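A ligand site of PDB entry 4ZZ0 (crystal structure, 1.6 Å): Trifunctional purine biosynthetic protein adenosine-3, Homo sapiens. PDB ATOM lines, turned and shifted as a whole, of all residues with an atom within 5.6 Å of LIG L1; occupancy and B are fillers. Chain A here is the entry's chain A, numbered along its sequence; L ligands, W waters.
The backbone NH (N) of Ser 13 is in hydrogen-bond range of an oxygen (O6) of LIG L1, 2.9 Å away. O6 of LIG L1 lies within hydrogen-bond range of OG of Ser 13. An oxygen (O2) of LIG L1 is in hydrogen-bond range of the side-chain carboxylate (OE1) of Glu 174 (2.7 Å). O7 of LIG L1 lies within hydrogen-bond range of N of Gly 12, 2.9 Å away. The backbone NH (N) of Asn 14 is in hydrogen-bond range of an oxygen (O8) of LIG L1, at 3.0 Å. O8 of LIG L1 sits at hydrogen-bond distance from ND2 of Asn 14 (3.0 Å). The side-chain amino group of Lys 171 lies within salt-bridge range of an oxygen (O6) of LIG L1 (3.3 Å). N of Asp 145 is in hydrogen-bond range of O1 of LG2 L2 (3.1 Å).
The side-chain hydroxyl of Ser 13 lies within hydrogen-bond range of a ring nitrogen (NE2) of His 175. The side-chain carboxylate (OE1) of Glu 174 lies within hydrogen-bond range of the side-chain amide nitrogen (ND2) of Asn 14. O of Lys 171 lies close to ND1 of His 175 (3.2 Å). The side-chain carboxylate (OD2) of Asp 145 sits close to a ring nitrogen (ND1) of His 109 (3.4 Å). The backbone NH (N) of Gly 118 lies within hydrogen-bond range of the side-chain carboxylate (OD2) of Asp 145 (2.9 Å).
Thr 11 touches LIG L1. Gly 88 touches LIG L1 (CA to C5, 3.6 Å). Met 90 touches LIG L1 (SD to C7, 3.8 Å). O of Ile 108 touches O2 of LIG L1, 3.7 Å away. His 109 touches LIG L1. Pro 110 touches LIG L1 (CD to O2, 3.3 Å). Gly 118 touches LIG L1. Hydrophobic or aromatic side chains within 4 Å of LIG L1: Met 90, Ile 108 and Pro 110. Of the 21 residues printed, 12 come within 4 Å of LIG L1. The nearest printed residue that does not touch LIG L1 is Gly 10 (4.1 Å).
Water W4 lies within hydrogen-bond range of O7 of LIG L1 (2.6 Å) and N of Thr 11 (3.0 Å). Water W1 lies within hydrogen-bond range of the side-chain carboxylate of Asp 145, a nitrogen (N2) of LIG L1, a ring nitrogen (ND1) of His 109 and the side-chain amide nitrogen of Asn 107. Water W8 lies within hydrogen-bond range of O1 of LIG L1 and NE2 of His 122. Water W2 lies within hydrogen-bond range of O7 of LIG L1 (2.8 Å), O of Ala 87 (2.8 Å), N of Gly 10 (3.0 Å) and O of Gly 88 (3.4 Å). Water W5 lies within hydrogen-bond range of the backbone carbonyl oxygen of Ile 108 (2.7 Å), a nitrogen (N1) of LIG L1 (2.8 Å) and the backbone NH of Gly 88 (2.9 Å). Water W3 lies within hydrogen-bond range of OE2 of Glu 174, NE2 of His 122 and O1 of LIG L1.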
ATOM      1  N   GLY A  10      13.210  12.039  -7.280  1.00  0.00           N
ATOM      2  CA  GLY A  10      11.919  11.494  -7.638  1.00  0.00           C
ATOM      3  C   GLY A  10      10.821  12.452  -8.039  1.00  0.00           C
ATOM      4  O   GLY A  10      11.010  13.320  -8.892  1.00  0.00           O
ATOM      5  N   THR A  11       9.663  12.282  -7.408  1.00  0.00           N
ATOM      6  CA  THR A  11       8.434  12.964  -7.791  1.00  0.00           C
ATOM      7  C   THR A  11       8.540  14.484  -7.747  1.00  0.00           C
ATOM      8  O   THR A  11       8.092  15.184  -8.660  1.00  0.00           O
ATOM      9  CB  THR A  11       7.272  12.511  -6.891  1.00  0.00           C
ATOM     10  OG1 THR A  11       7.118  11.091  -7.037  1.00  0.00           O
ATOM     11  CG2 THR A  11       5.978  13.206  -7.286  1.00  0.00           C
ATOM     12  N   GLY A  12       9.135  15.002  -6.678  1.00  0.00           N
ATOM     13  CA  GLY A  12       9.356  16.419  -6.568  1.00  0.00           C
ATOM     14  C   GLY A  12       8.214  17.249  -5.994  1.00  0.00           C
ATOM     15  O   GLY A  12       8.109  18.441  -6.294  1.00  0.00           O
ATOM     16  N   SER A  13       7.356  16.649  -5.166  1.00  0.00           N
ATOM     17  CA  SER A  13       6.316  17.469  -4.550  1.00  0.00           C
ATOM     18  C   SER A  13       6.925  18.489  -3.584  1.00  0.00           C
ATOM     19  O   SER A  13       6.432  19.617  -3.490  1.00  0.00           O
ATOM     20  CB  SER A  13       5.271  16.600  -3.818  1.00  0.00           C
ATOM     21  OG  SER A  13       5.807  16.009  -2.641  1.00  0.00           O
ATOM     22  N   ASN A  14       7.991  18.129  -2.877  1.00  0.00           N
ATOM     23  CA  ASN A  14       8.650  19.112  -2.017  1.00  0.00           C
ATOM     24  C   ASN A  14       9.282  20.203  -2.847  1.00  0.00           C
ATOM     25  O   ASN A  14       9.200  21.378  -2.496  1.00  0.00           O
ATOM     26  CB  ASN A  14       9.683  18.455  -1.099  1.00  0.00           C
ATOM     27  CG  ASN A  14       9.069  17.902   0.176  1.00  0.00           C
ATOM     28  OD1 ASN A  14       8.704  18.651   1.072  1.00  0.00           O
ATOM     29  ND2 ASN A  14       8.967  16.588   0.265  1.00  0.00           N
ATOM     30  N   LEU A  15       9.926  19.820  -3.947  1.00  0.00           N
ATOM     31  CA  LEU A  15      10.460  20.819  -4.879  1.00  0.00           C
ATOM     32  C   LEU A  15       9.372  21.801  -5.305  1.00  0.00           C
ATOM     33  O   LEU A  15       9.590  23.003  -5.299  1.00  0.00           O
ATOM     34  CB  LEU A  15      11.056  20.158  -6.108  1.00  0.00           C
ATOM     35  CG  LEU A  15      11.332  21.075  -7.307  1.00  0.00           C
ATOM     36  CD1 LEU A  15      12.385  22.115  -6.933  1.00  0.00           C
ATOM     37  CD2 LEU A  15      11.788  20.243  -8.501  1.00  0.00           C
ATOM     38  N   ALA A  87      15.577  17.392  -1.298  1.00  0.00           N
ATOM     39  CA  ALA A  87      14.126  17.284  -1.341  1.00  0.00           C
ATOM     40  C   ALA A  87      13.763  15.978  -2.014  1.00  0.00           C
ATOM     41  O   ALA A  87      13.539  15.921  -3.228  1.00  0.00           O
ATOM     42  CB  ALA A  87      13.519  18.481  -2.075  1.00  0.00           C
ATOM     43  N   GLY A  88      13.734  14.914  -1.217  1.00  0.00           N
ATOM     44  CA  GLY A  88      13.593  13.571  -1.755  1.00  0.00           C
ATOM     45  C   GLY A  88      14.824  13.056  -2.475  1.00  0.00           C
ATOM     46  O   GLY A  88      14.734  12.123  -3.261  1.00  0.00           O
ATOM     47  N   PHE A  89      15.982  13.674  -2.211  1.00  0.00           N
ATOM     48  CA  PHE A  89      17.272  13.224  -2.707  1.00  0.00           C
ATOM     49  C   PHE A  89      17.738  12.050  -1.846  1.00  0.00           C
ATOM     50  O   PHE A  89      17.894  12.199  -0.639  1.00  0.00           O
ATOM     51  CB  PHE A  89      18.286  14.382  -2.679  1.00  0.00           C
ATOM     52  CG  PHE A  89      19.644  14.028  -3.203  1.00  0.00           C
ATOM     53  CD1 PHE A  89      19.870  13.947  -4.559  1.00  0.00           C
ATOM     54  CD2 PHE A  89      20.707  13.821  -2.339  1.00  0.00           C
ATOM     55  CE1 PHE A  89      21.128  13.650  -5.059  1.00  0.00           C
ATOM     56  CE2 PHE A  89      21.968  13.516  -2.818  1.00  0.00           C
ATOM     57  CZ  PHE A  89      22.175  13.426  -4.178  1.00  0.00           C
ATOM     58  N   MET A  90      17.954  10.889  -2.444  1.00  0.00           N
ATOM     59  CA  MET A  90      18.138   9.688  -1.646  1.00  0.00           C
ATOM     60  C   MET A  90      19.547   9.130  -1.675  1.00  0.00           C
ATOM     61  O   MET A  90      19.752   7.914  -1.675  1.00  0.00           O
ATOM     62  CB  MET A  90      17.147   8.613  -2.114  1.00  0.00           C
ATOM     63  CG  MET A  90      15.675   9.022  -2.019  1.00  0.00           C
ATOM     64  SD  MET A  90      15.161   9.552  -0.374  1.00  0.00           S
ATOM     65  CE  MET A  90      15.220   8.000   0.519  1.00  0.00           C
ATOM     66  N   ASN A 107      17.777  19.207   4.858  1.00  0.00           N
ATOM     67  CA  ASN A 107      17.129  17.970   4.407  1.00  0.00           C
ATOM     68  C   ASN A 107      15.747  17.851   5.005  1.00  0.00           C
ATOM     69  O   ASN A 107      15.536  18.269   6.139  1.00  0.00           O
ATOM     70  CB  ASN A 107      17.953  16.746   4.806  1.00  0.00           C
ATOM     71  CG  ASN A 107      17.326  15.433   4.342  1.00  0.00           C
ATOM     72  OD1 ASN A 107      17.085  15.229   3.152  1.00  0.00           O
ATOM     73  ND2 ASN A 107      17.084  14.516   5.292  1.00  0.00           N
ATOM     74  N   ILE A 108      14.813  17.266   4.247  1.00  0.00           N
ATOM     75  CA  ILE A 108      13.497  16.931   4.797  1.00  0.00           C
ATOM     76  C   ILE A 108      13.427  15.420   5.008  1.00  0.00           C
ATOM     77  O   ILE A 108      13.883  14.620   4.188  1.00  0.00           O
ATOM     78  CB  ILE A 108      12.325  17.432   3.896  1.00  0.00           C
ATOM     79  CG1 ILE A 108      10.961  17.113   4.520  1.00  0.00           C
ATOM     80  CG2 ILE A 108      12.357  16.811   2.530  1.00  0.00           C
ATOM     81  CD1 ILE A 108      10.406  18.168   5.384  1.00  0.00           C
ATOM     82  N   HIS A 109      12.874  15.019   6.157  1.00  0.00           N
ATOM     83  CA  HIS A 109      12.805  13.614   6.502  1.00  0.00           C
ATOM     84  C   HIS A 109      11.410  13.345   7.072  1.00  0.00           C
ATOM     85  O   HIS A 109      10.956  14.101   7.909  1.00  0.00           O
ATOM     86  CB  HIS A 109      13.872  13.247   7.537  1.00  0.00           C
ATOM     87  CG  HIS A 109      13.853  11.802   7.940  1.00  0.00           C
ATOM     88  ND1 HIS A 109      14.452  10.809   7.203  1.00  0.00           N
ATOM     89  CD2 HIS A 109      13.286  11.190   9.003  1.00  0.00           C
ATOM     90  CE1 HIS A 109      14.256   9.642   7.790  1.00  0.00           C
ATOM     91  NE2 HIS A 109      13.560   9.847   8.894  1.00  0.00           N
ATOM     92  N   PRO A 110      10.747  12.278   6.603  1.00  0.00           N
ATOM     93  CA  PRO A 110       9.339  12.085   6.962  1.00  0.00           C
ATOM     94  C   PRO A 110       9.120  11.305   8.259  1.00  0.00           C
ATOM     95  O   PRO A 110       8.351  10.340   8.301  1.00  0.00           O
ATOM     96  CB  PRO A 110       8.780  11.330   5.765  1.00  0.00           C
ATOM     97  CG  PRO A 110       9.956  10.429   5.366  1.00  0.00           C
ATOM     98  CD  PRO A 110      11.185  11.334   5.550  1.00  0.00           C
ATOM     99  N   GLY A 118      16.538   6.880   8.601  1.00  0.00           N
ATOM    100  CA  GLY A 118      16.705   5.984   7.463  1.00  0.00           C
ATOM    101  C   GLY A 118      15.714   6.154   6.323  1.00  0.00           C
ATOM    102  O   GLY A 118      14.983   7.132   6.260  1.00  0.00           O
ATOM    103  N   SER A 119      15.672   5.163   5.419  1.00  0.00           N
ATOM    104  CA  SER A 119      15.011   5.317   4.122  1.00  0.00           C
ATOM    105  C   SER A 119      13.527   4.985   4.051  1.00  0.00           C
ATOM    106  O   SER A 119      12.844   5.398   3.102  1.00  0.00           O
ATOM    107  CB  SER A 119      15.722   4.430   3.091  1.00  0.00           C
ATOM    108  OG  SER A 119      15.627   3.082   3.487  1.00  0.00           O
ATOM    109  N   HIS A 122       8.169   5.653   7.110  1.00  0.00           N
ATOM    110  CA  HIS A 122       6.751   5.320   7.299  1.00  0.00           C
ATOM    111  C   HIS A 122       6.562   3.842   7.632  1.00  0.00           C
ATOM    112  O   HIS A 122       5.723   3.495   8.468  1.00  0.00           O
ATOM    113  CB  HIS A 122       5.918   5.654   6.054  1.00  0.00           C
ATOM    114  CG  HIS A 122       5.946   7.104   5.705  1.00  0.00           C
ATOM    115  ND1 HIS A 122       5.566   8.095   6.601  1.00  0.00           N
ATOM    116  CD2 HIS A 122       6.294   7.734   4.565  1.00  0.00           C
ATOM    117  CE1 HIS A 122       5.703   9.267   6.012  1.00  0.00           C
ATOM    118  NE2 HIS A 122       6.126   9.084   4.781  1.00  0.00           N
ATOM    119  N   ASP A 145      20.670  11.889   9.218  1.00  0.00           N
ATOM    120  CA  ASP A 145      19.455  12.219   9.965  1.00  0.00           C
ATOM    121  C   ASP A 145      19.745  12.613  11.420  1.00  0.00           C
ATOM    122  O   ASP A 145      18.868  12.530  12.283  1.00  0.00           O
ATOM    123  CB  ASP A 145      18.463  11.037   9.919  1.00  0.00           C
ATOM    124  CG  ASP A 145      17.950  10.774   8.511  1.00  0.00           C
ATOM    125  OD1 ASP A 145      18.039  11.679   7.661  1.00  0.00           O
ATOM    126  OD2 ASP A 145      17.446   9.656   8.267  1.00  0.00           O
ATOM    127  N   LYS A 171       3.150  14.379   3.723  1.00  0.00           N
ATOM    128  CA  LYS A 171       3.638  15.320   2.705  1.00  0.00           C
ATOM    129  C   LYS A 171       2.931  16.678   2.785  1.00  0.00           C
ATOM    130  O   LYS A 171       3.531  17.698   2.425  1.00  0.00           O
ATOM    131  CB  LYS A 171       3.500  14.721   1.304  1.00  0.00           C
ATOM    132  CG  LYS A 171       4.671  13.793   0.973  1.00  0.00           C
ATOM    133  CD  LYS A 171       4.593  13.239  -0.431  1.00  0.00           C
ATOM    134  CE  LYS A 171       5.768  12.308  -0.710  1.00  0.00           C
ATOM    135  NZ  LYS A 171       5.749  11.885  -2.151  1.00  0.00           N
ATOM    136  N   GLU A 174       5.085  18.357   5.160  1.00  0.00           N
ATOM    137  CA  GLU A 174       6.412  18.589   4.582  1.00  0.00           C
ATOM    138  C   GLU A 174       6.388  19.856   3.752  1.00  0.00           C
ATOM    139  O   GLU A 174       7.316  20.665   3.801  1.00  0.00           O
ATOM    140  CB  GLU A 174       6.853  17.420   3.703  1.00  0.00           C
ATOM    141  CG  GLU A 174       7.053  16.117   4.454  1.00  0.00           C
ATOM    142  CD  GLU A 174       7.590  15.019   3.561  1.00  0.00           C
ATOM    143  OE1 GLU A 174       8.467  15.314   2.718  1.00  0.00           O
ATOM    144  OE2 GLU A 174       7.147  13.864   3.685  1.00  0.00           O
ATOM    145  N   HIS A 175       5.301  20.037   3.004  1.00  0.00           N
ATOM    146  CA  HIS A 175       5.173  21.159   2.097  1.00  0.00           C
ATOM    147  C   HIS A 175       4.954  22.484   2.813  1.00  0.00           C
ATOM    148  O   HIS A 175       5.017  23.542   2.197  1.00  0.00           O
ATOM    149  CB  HIS A 175       4.035  20.912   1.122  1.00  0.00           C
ATOM    150  CG  HIS A 175       4.232  19.700   0.279  1.00  0.00           C
ATOM    151  ND1 HIS A 175       3.199  19.114  -0.428  1.00  0.00           N
ATOM    152  CD2 HIS A 175       5.331  18.942   0.051  1.00  0.00           C
ATOM    153  CE1 HIS A 175       3.659  18.060  -1.066  1.00  0.00           C
ATOM    154  NE2 HIS A 175       4.950  17.923  -0.794  1.00  0.00           N
HETATM  155  C1  LIG L   1       9.394  12.894   0.992  1.00  0.00           C
HETATM  156  O1  LIG L   1       8.391  12.254   1.806  1.00  0.00           O
HETATM  157  C2  LIG L   1      10.667  13.070   1.794  1.00  0.00           C
HETATM  158  O2  LIG L   1      10.471  13.498   3.148  1.00  0.00           O
HETATM  159  C3  LIG L   1      11.281  11.678   1.721  1.00  0.00           C
HETATM  160  O3  LIG L   1      11.054  11.330   0.356  1.00  0.00           O
HETATM  161  C4  LIG L   1       9.831  11.924  -0.105  1.00  0.00           C
HETATM  162  C5  LIG L   1      10.105  12.676  -1.403  1.00  0.00           C
HETATM  163  O4  LIG L   1       8.890  13.129  -1.989  1.00  0.00           O
HETATM  164  N1  LIG L   1      12.692  11.714   2.015  1.00  0.00           N
HETATM  165  C6  LIG L   1      13.285  10.753   2.718  1.00  0.00           C
HETATM  166  O5  LIG L   1      12.730   9.720   3.046  1.00  0.00           O
HETATM  167  C7  LIG L   1      14.720  11.030   3.102  1.00  0.00           C
HETATM  168  N2  LIG L   1      15.297   9.909   3.827  1.00  0.00           N
HETATM  169  P1  LIG L   1       8.908  14.225  -3.175  1.00  0.00           P
HETATM  170  O6  LIG L   1       7.460  14.265  -3.603  1.00  0.00           O
HETATM  171  O7  LIG L   1       9.901  13.682  -4.185  1.00  0.00           O
HETATM  172  O8  LIG L   1       9.390  15.499  -2.530  1.00  0.00           O
HETATM  173  N1  LG2 L   2      23.967  12.544   3.873  1.00  0.00           N
HETATM  174  C1  LG2 L   2      24.543  12.821   5.090  1.00  0.00           C
HETATM  175  N2  LG2 L   2      23.767  13.225   6.154  1.00  0.00           N
HETATM  176  C2  LG2 L   2      22.402  13.342   6.028  1.00  0.00           C
HETATM  177  N3  LG2 L   2      21.769  12.430   2.613  1.00  0.00           N
HETATM  178  C3  LG2 L   2      20.534  12.673   3.009  1.00  0.00           C
HETATM  179  C4  LG2 L   2      20.508  13.053   4.251  1.00  0.00           C
HETATM  180  C5  LG2 L   2      21.773  13.060   4.789  1.00  0.00           C
HETATM  181  C6  LG2 L   2      22.632  12.645   3.721  1.00  0.00           C
HETATM  182  O1  LG2 L   2      21.781  13.701   7.008  1.00  0.00           O
HETATM  183  N4  LG2 L   2      25.941  12.700   5.234  1.00  0.00           N
HETATM  184  C7  LG2 L   2      18.769   5.190   1.821  1.00  0.00           C
HETATM  185  C8  LG2 L   2      19.195   6.360   2.741  1.00  0.00           C
HETATM  186  C9  LG2 L   2      19.243   7.632   1.876  1.00  0.00           C
HETATM  187  C10 LG2 L   2      19.948   4.773   0.924  1.00  0.00           C
HETATM  188  O2  LG2 L   2      19.708   4.232  -0.154  1.00  0.00           O
HETATM  189  N5  LG2 L   2      21.299   5.024   1.400  1.00  0.00           N
HETATM  190  C11 LG2 L   2      22.506   4.686   0.660  1.00  0.00           C
HETATM  191  C12 LG2 L   2      22.542   3.202   0.353  1.00  0.00           C
HETATM  192  C13 LG2 L   2      22.270   2.416   1.627  1.00  0.00           C
HETATM  193  C14 LG2 L   2      21.253   1.344   1.370  1.00  0.00           C
HETATM  194  O3  LG2 L   2      20.863   1.113   0.176  1.00  0.00           O
HETATM  195  O4  LG2 L   2      20.777   0.652   2.332  1.00  0.00           O
HETATM  196  C15 LG2 L   2      22.617   5.513  -0.603  1.00  0.00           C
HETATM  197  O5  LG2 L   2      23.565   6.350  -0.722  1.00  0.00           O
HETATM  198  O6  LG2 L   2      21.778   5.375  -1.535  1.00  0.00           O
HETATM  199  C16 LG2 L   2      19.300  12.559   2.099  1.00  0.00           C
HETATM  200  C17 LG2 L   2      18.518  11.322   2.441  1.00  0.00           C
HETATM  201  C18 LG2 L   2      19.364  10.114   2.117  1.00  0.00           C
HETATM  202  C19 LG2 L   2      18.696   8.849   2.686  1.00  0.00           C
HETATM  203  O   HOH W   1      16.492  11.603   5.527  1.00  0.00           O
HETATM  204  O   HOH W   2      12.526  14.024  -5.072  1.00  0.00           O
HETATM  205  O   HOH W   3       5.654  11.647   3.660  1.00  0.00           O
HETATM  206  O   HOH W   4      10.041  11.096  -4.688  1.00  0.00           O
HETATM  207  O   HOH W   5      14.116  14.111   1.540  1.00  0.00           O
HETATM  208  O   HOH W   6      11.471   9.025  -1.468  1.00  0.00           O
HETATM  209  O   HOH W   7      10.965  17.094  -3.963  1.00  0.00           O
HETATM  210  O   HOH W   8       7.686   9.633   1.931  1.00  0.00           O
HETATM  211  O   HOH W   9      12.270   7.688   5.045  1.00  0.00           O
